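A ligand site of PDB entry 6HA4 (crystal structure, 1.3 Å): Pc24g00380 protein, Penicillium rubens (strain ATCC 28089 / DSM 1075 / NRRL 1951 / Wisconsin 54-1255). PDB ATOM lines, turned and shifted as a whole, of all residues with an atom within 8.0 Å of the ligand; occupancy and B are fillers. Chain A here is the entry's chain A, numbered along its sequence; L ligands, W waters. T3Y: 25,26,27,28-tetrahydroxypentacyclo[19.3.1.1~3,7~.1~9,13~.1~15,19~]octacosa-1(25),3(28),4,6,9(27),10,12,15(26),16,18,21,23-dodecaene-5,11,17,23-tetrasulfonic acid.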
ATOM      1  N   LYS A  11     -15.942 -22.760   8.144  1.00  0.00           N
ATOM      2  CA  LYS A  11     -15.178 -23.700   7.322  1.00  0.00           C
ATOM      3  C   LYS A  11     -15.393 -23.445   5.819  1.00  0.00           C
ATOM      4  O   LYS A  11     -14.679 -24.012   4.992  1.00  0.00           O
ATOM      5  CB  LYS A  11     -15.560 -25.144   7.657  1.00  0.00           C
ATOM      6  CG  LYS A  11     -15.113 -25.593   9.037  1.00  0.00           C
ATOM      7  CD  LYS A  11     -15.629 -26.989   9.320  1.00  0.00           C
ATOM      8  CE  LYS A  11     -14.995 -27.624  10.529  1.00  0.00           C
ATOM      9  NZ  LYS A  11     -15.608 -28.946  10.821  1.00  0.00           N
ATOM     10  N   ASN A  12     -16.383 -22.614   5.472  1.00  0.00           N
ATOM     11  CA  ASN A  12     -16.760 -22.351   4.091  1.00  0.00           C
ATOM     12  C   ASN A  12     -16.986 -23.651   3.330  1.00  0.00           C
ATOM     13  O   ASN A  12     -16.452 -23.840   2.243  1.00  0.00           O
ATOM     14  CB  ASN A  12     -15.705 -21.492   3.385  1.00  0.00           C
ATOM     15  CG  ASN A  12     -16.243 -20.843   2.133  1.00  0.00           C
ATOM     16  OD1 ASN A  12     -17.454 -20.643   1.984  1.00  0.00           O
ATOM     17  ND2 ASN A  12     -15.371 -20.545   1.189  1.00  0.00           N
ATOM     18  N   LYS A  27     -15.565 -28.078  -0.214  1.00  0.00           N
ATOM     19  CA  LYS A  27     -15.154 -26.701  -0.004  1.00  0.00           C
ATOM     20  C   LYS A  27     -15.908 -25.777  -0.959  1.00  0.00           C
ATOM     21  O   LYS A  27     -15.961 -26.040  -2.165  1.00  0.00           O
ATOM     22  CB  LYS A  27     -13.634 -26.607  -0.241  1.00  0.00           C
ATOM     23  CG  LYS A  27     -12.987 -25.262   0.014  1.00  0.00           C
ATOM     24  CD  LYS A  27     -13.467 -24.605   1.283  1.00  0.00           C
ATOM     25  CE  LYS A  27     -12.555 -23.485   1.706  1.00  0.00           C
ATOM     26  NZ  LYS A  27     -12.416 -22.448   0.649  1.00  0.00           N
ATOM     27  N   CYS A  28     -16.526 -24.708  -0.435  1.00  0.00           N
ATOM     28  CA  CYS A  28     -17.051 -23.651  -1.299  1.00  0.00           C
ATOM     29  C   CYS A  28     -15.844 -22.924  -1.872  1.00  0.00           C
ATOM     30  O   CYS A  28     -14.843 -22.757  -1.158  1.00  0.00           O
ATOM     31  CB  CYS A  28     -17.924 -22.658  -0.526  1.00  0.00           C
ATOM     32  SG  CYS A  28     -19.289 -23.393   0.418  1.00  0.00           S
ATOM     33  N   PRO A  29     -15.995 -22.250  -3.006  1.00  0.00           N
ATOM     34  CA  PRO A  29     -14.937 -21.336  -3.467  1.00  0.00           C
ATOM     35  C   PRO A  29     -14.766 -20.164  -2.510  1.00  0.00           C
ATOM     36  O   PRO A  29     -15.702 -19.799  -1.796  1.00  0.00           O
ATOM     37  CB  PRO A  29     -15.442 -20.864  -4.826  1.00  0.00           C
ATOM     38  CG  PRO A  29     -16.415 -21.926  -5.270  1.00  0.00           C
ATOM     39  CD  PRO A  29     -17.092 -22.328  -4.002  1.00  0.00           C
ATOM     40  N   LYS A  30     -13.574 -19.548  -2.516  1.00  0.00           N
ATOM     41  CA  LYS A  30     -13.357 -18.321  -1.759  1.00  0.00           C
ATOM     42  C   LYS A  30     -14.061 -17.142  -2.444  1.00  0.00           C
ATOM     43  O   LYS A  30     -14.502 -16.217  -1.756  1.00  0.00           O
ATOM     44  CB  LYS A  30     -11.852 -18.038  -1.615  1.00  0.00           C
ATOM     45  CG  LYS A  30     -11.550 -16.693  -0.986  1.00  0.00           C
ATOM     46  CD  LYS A  30     -10.073 -16.528  -0.706  1.00  0.00           C
ATOM     47  CE  LYS A  30      -9.774 -15.254   0.049  1.00  0.00           C
ATOM     48  NZ  LYS A  30     -10.391 -15.246   1.406  1.00  0.00           N
ATOM     49  N   PHE A  31     -14.144 -17.152  -3.784  1.00  0.00           N
ATOM     50  CA  PHE A  31     -14.739 -16.039  -4.520  1.00  0.00           C
ATOM     51  C   PHE A  31     -16.052 -15.590  -3.885  1.00  0.00           C
ATOM     52  O   PHE A  31     -16.895 -16.430  -3.600  1.00  0.00           O
ATOM     53  CB  PHE A  31     -14.951 -16.403  -5.993  1.00  0.00           C
ATOM     54  CG  PHE A  31     -13.691 -16.351  -6.824  1.00  0.00           C
ATOM     55  CD1 PHE A  31     -12.981 -15.166  -6.970  1.00  0.00           C
ATOM     56  CD2 PHE A  31     -13.250 -17.466  -7.516  1.00  0.00           C
ATOM     57  CE1 PHE A  31     -11.826 -15.125  -7.737  1.00  0.00           C
ATOM     58  CE2 PHE A  31     -12.095 -17.424  -8.283  1.00  0.00           C
ATOM     59  CZ  PHE A  31     -11.395 -16.248  -8.402  1.00  0.00           C
ATOM     60  N   ASP A  32     -16.205 -14.275  -3.655  1.00  0.00           N
ATOM     61  CA  ASP A  32     -17.342 -13.717  -2.915  1.00  0.00           C
ATOM     62  C   ASP A  32     -18.694 -14.258  -3.350  1.00  0.00           C
ATOM     63  O   ASP A  32     -19.505 -14.597  -2.506  1.00  0.00           O
ATOM     64  CB  ASP A  32     -17.359 -12.186  -3.040  1.00  0.00           C
ATOM     65  CG  ASP A  32     -16.251 -11.482  -2.299  1.00  0.00           C
ATOM     66  OD1 ASP A  32     -15.719 -12.069  -1.332  1.00  0.00           O
ATOM     67  OD2 ASP A  32     -15.927 -10.335  -2.664  1.00  0.00           O
ATOM     68  N   ASN A  33     -18.945 -14.310  -4.664  1.00  0.00           N
ATOM     69  CA  ASN A  33     -20.264 -14.679  -5.177  1.00  0.00           C
ATOM     70  C   ASN A  33     -20.581 -16.181  -5.033  1.00  0.00           C
ATOM     71  O   ASN A  33     -21.713 -16.579  -5.299  1.00  0.00           O
ATOM     72  CB  ASN A  33     -20.430 -14.229  -6.632  1.00  0.00           C
ATOM     73  CG  ASN A  33     -19.621 -15.008  -7.637  1.00  0.00           C
ATOM     74  OD1 ASN A  33     -18.546 -15.542  -7.329  1.00  0.00           O
ATOM     75  ND2 ASN A  33     -20.111 -15.086  -8.864  1.00  0.00           N
ATOM     76  N   LYS A  34     -19.596 -17.000  -4.637  1.00  0.00           N
ATOM     77  CA  LYS A  34     -19.810 -18.438  -4.456  1.00  0.00           C
ATOM     78  C   LYS A  34     -19.472 -18.916  -3.035  1.00  0.00           C
ATOM     79  O   LYS A  34     -19.553 -20.107  -2.766  1.00  0.00           O
ATOM     80  CB  LYS A  34     -18.940 -19.216  -5.467  1.00  0.00           C
ATOM     81  CG  LYS A  34     -19.348 -19.036  -6.926  1.00  0.00           C
ATOM     82  CD  LYS A  34     -18.195 -19.404  -7.852  1.00  0.00           C
ATOM     83  CE  LYS A  34     -18.629 -19.867  -9.215  1.00  0.00           C
ATOM     84  NZ  LYS A  34     -17.604 -20.750  -9.829  1.00  0.00           N
ATOM     85  N   LYS A  35     -19.068 -18.002  -2.137  1.00  0.00           N
ATOM     86  CA  LYS A  35     -18.662 -18.396  -0.790  1.00  0.00           C
ATOM     87  C   LYS A  35     -19.842 -18.470   0.166  1.00  0.00           C
ATOM     88  O   LYS A  35     -20.836 -17.758  -0.006  1.00  0.00           O
ATOM     89  CB  LYS A  35     -17.592 -17.424  -0.248  1.00  0.00           C
ATOM     90  CG  LYS A  35     -18.119 -16.384   0.745  1.00  0.00           C
ATOM     91  CD  LYS A  35     -17.188 -15.191   0.929  1.00  0.00           C
ATOM     92  CE  LYS A  35     -15.708 -15.523   0.963  1.00  0.00           C
ATOM     93  NZ  LYS A  35     -14.875 -14.493   0.280  1.00  0.00           N
HETATM   94  O3  T3Y L   1     -10.831 -20.535  -6.364  1.00  0.00           O
HETATM   95  S1  T3Y L   1     -11.130 -19.840  -5.090  1.00  0.00           S
HETATM   96  O1  T3Y L   1     -11.236 -20.817  -3.999  1.00  0.00           O
HETATM   97  O2  T3Y L   1     -12.414 -19.136  -5.252  1.00  0.00           O
HETATM   98  C1  T3Y L   1      -9.926 -18.805  -4.779  1.00  0.00           C
HETATM   99  C24 T3Y L   1      -9.991 -17.470  -5.215  1.00  0.00           C
HETATM  100  C23 T3Y L   1      -8.930 -16.574  -5.019  1.00  0.00           C
HETATM  101  C22 T3Y L   1      -9.039 -15.136  -5.509  1.00  0.00           C
HETATM  102  C2  T3Y L   1      -8.770 -19.297  -4.158  1.00  0.00           C
HETATM  103  C3  T3Y L   1      -7.655 -18.495  -3.936  1.00  0.00           C
HETATM  104  C25 T3Y L   1      -7.677 -17.086  -4.400  1.00  0.00           C
HETATM  105  O13 T3Y L   1      -6.585 -16.295  -4.238  1.00  0.00           O
HETATM  106  C4  T3Y L   1      -6.428 -19.047  -3.249  1.00  0.00           C
HETATM  107  C5  T3Y L   1      -6.441 -18.656  -1.779  1.00  0.00           C
HETATM  108  C6  T3Y L   1      -7.179 -19.386  -0.862  1.00  0.00           C
HETATM  109  C7  T3Y L   1      -7.237 -19.029   0.480  1.00  0.00           C
HETATM  110  S2  T3Y L   1      -8.102 -19.939   1.468  1.00  0.00           S
HETATM  111  O4  T3Y L   1      -9.511 -19.950   1.016  1.00  0.00           O
HETATM  112  O5  T3Y L   1      -7.598 -21.331   1.428  1.00  0.00           O
HETATM  113  O6  T3Y L   1      -8.045 -19.421   2.851  1.00  0.00           O
HETATM  114  C8  T3Y L   1      -6.525 -17.927   0.975  1.00  0.00           C
HETATM  115  C28 T3Y L   1      -5.706 -17.449  -1.307  1.00  0.00           C
HETATM  116  O16 T3Y L   1      -4.958 -16.687  -2.143  1.00  0.00           O
HETATM  117  C9  T3Y L   1      -5.768 -17.104   0.135  1.00  0.00           C
HETATM  118  C10 T3Y L   1      -5.018 -15.894   0.666  1.00  0.00           C
HETATM  119  C11 T3Y L   1      -5.921 -14.676   0.668  1.00  0.00           C
HETATM  120  C12 T3Y L   1      -6.529 -14.272   1.856  1.00  0.00           C
HETATM  121  C13 T3Y L   1      -7.403 -13.184   1.903  1.00  0.00           C
HETATM  122  S3  T3Y L   1      -8.058 -12.754   3.292  1.00  0.00           S
HETATM  123  O7  T3Y L   1      -7.308 -13.346   4.426  1.00  0.00           O
HETATM  124  O8  T3Y L   1      -9.456 -13.225   3.309  1.00  0.00           O
HETATM  125  O9  T3Y L   1      -8.043 -11.273   3.406  1.00  0.00           O
HETATM  126  C14 T3Y L   1      -7.721 -12.464   0.746  1.00  0.00           C
HETATM  127  C27 T3Y L   1      -6.181 -13.902  -0.565  1.00  0.00           C
HETATM  128  O15 T3Y L   1      -5.543 -14.187  -1.732  1.00  0.00           O
HETATM  129  C15 T3Y L   1      -7.160 -12.777  -0.490  1.00  0.00           C
HETATM  130  C16 T3Y L   1      -7.484 -11.946  -1.715  1.00  0.00           C
HETATM  131  C17 T3Y L   1      -8.591 -12.586  -2.533  1.00  0.00           C
HETATM  132  C18 T3Y L   1      -9.940 -12.289  -2.306  1.00  0.00           C
HETATM  133  C26 T3Y L   1      -8.251 -13.507  -3.635  1.00  0.00           C
HETATM  134  O14 T3Y L   1      -6.949 -13.791  -3.932  1.00  0.00           O
HETATM  135  C21 T3Y L   1      -9.358 -14.187  -4.361  1.00  0.00           C
HETATM  136  C20 T3Y L   1     -10.675 -13.806  -4.070  1.00  0.00           C
HETATM  137  C19 T3Y L   1     -10.976 -12.912  -3.021  1.00  0.00           C
HETATM  138  S4  T3Y L   1     -12.506 -12.535  -2.682  1.00  0.00           S
HETATM  139  O11 T3Y L   1     -13.413 -13.080  -3.720  1.00  0.00           O
HETATM  140  O10 T3Y L   1     -12.651 -11.060  -2.655  1.00  0.00           O
HETATM  141  O12 T3Y L   1     -12.868 -13.123  -1.367  1.00  0.00           O
HETATM  142  O   HOH W   1      -8.891 -19.259  -8.337  1.00  0.00           O
HETATM  143  O   HOH W   2      -2.891 -17.151  -3.623  1.00  0.00           O
HETATM  144  O   HOH W   3     -11.049 -14.019   5.234  1.00  0.00           O
HETATM  145  O   HOH W   4      -5.259 -16.838  -6.779  1.00  0.00           O
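N of Lys 30 sits at hydrogen-bond distance from O2 of the ligand, at 3.0 Å. The side-chain amino group (NZ) of Lys 30 lies within salt-bridge range of an oxygen (O8) of the ligand (2.9 Å). An oxygen (O2) of the ligand lies close to the backbone NH (N) of Phe 31, at 3.0 Å. The side-chain amino group (NZ) of Lys 35 lies within salt-bridge range of an oxygen (O12) of the ligand, 2.9 Å away. The backbone NH (N) of Asp 32 lies within hydrogen-bond range of an oxygen (O11) of the ligand, at 3.0 Å. O12 of the ligand lies close to OD1 of Asp 32. NZ of Lys 27 is in salt-bridge range of O4 of the ligand (3.8 Å).
The backbone carbonyl oxygen (O) of Lys 30 is in hydrogen-bond range of the side-chain amino group (NZ) of Lys 35 (2.7 Å). NZ of Lys 35 is in salt-bridge range of OD1 of Asp 32, 3.0 Å away. The side-chain amide nitrogen (ND2) of Asn 12 sits at hydrogen-bond distance from the backbone carbonyl oxygen (O) of Pro 29.
Residues that only touch the ligand: Pro 29. Hydrophobic or aromatic side chains within 4 Å of the ligand: Pro 29 and Phe 31. Six residues have an atom within 4 Å of the ligand: Lys 27, Pro 29, Lys 30, Phe 31, Asp 32 and Lys 35. The nearest printed residue that does not touch the ligand is Cys 28 (5.0 Å).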
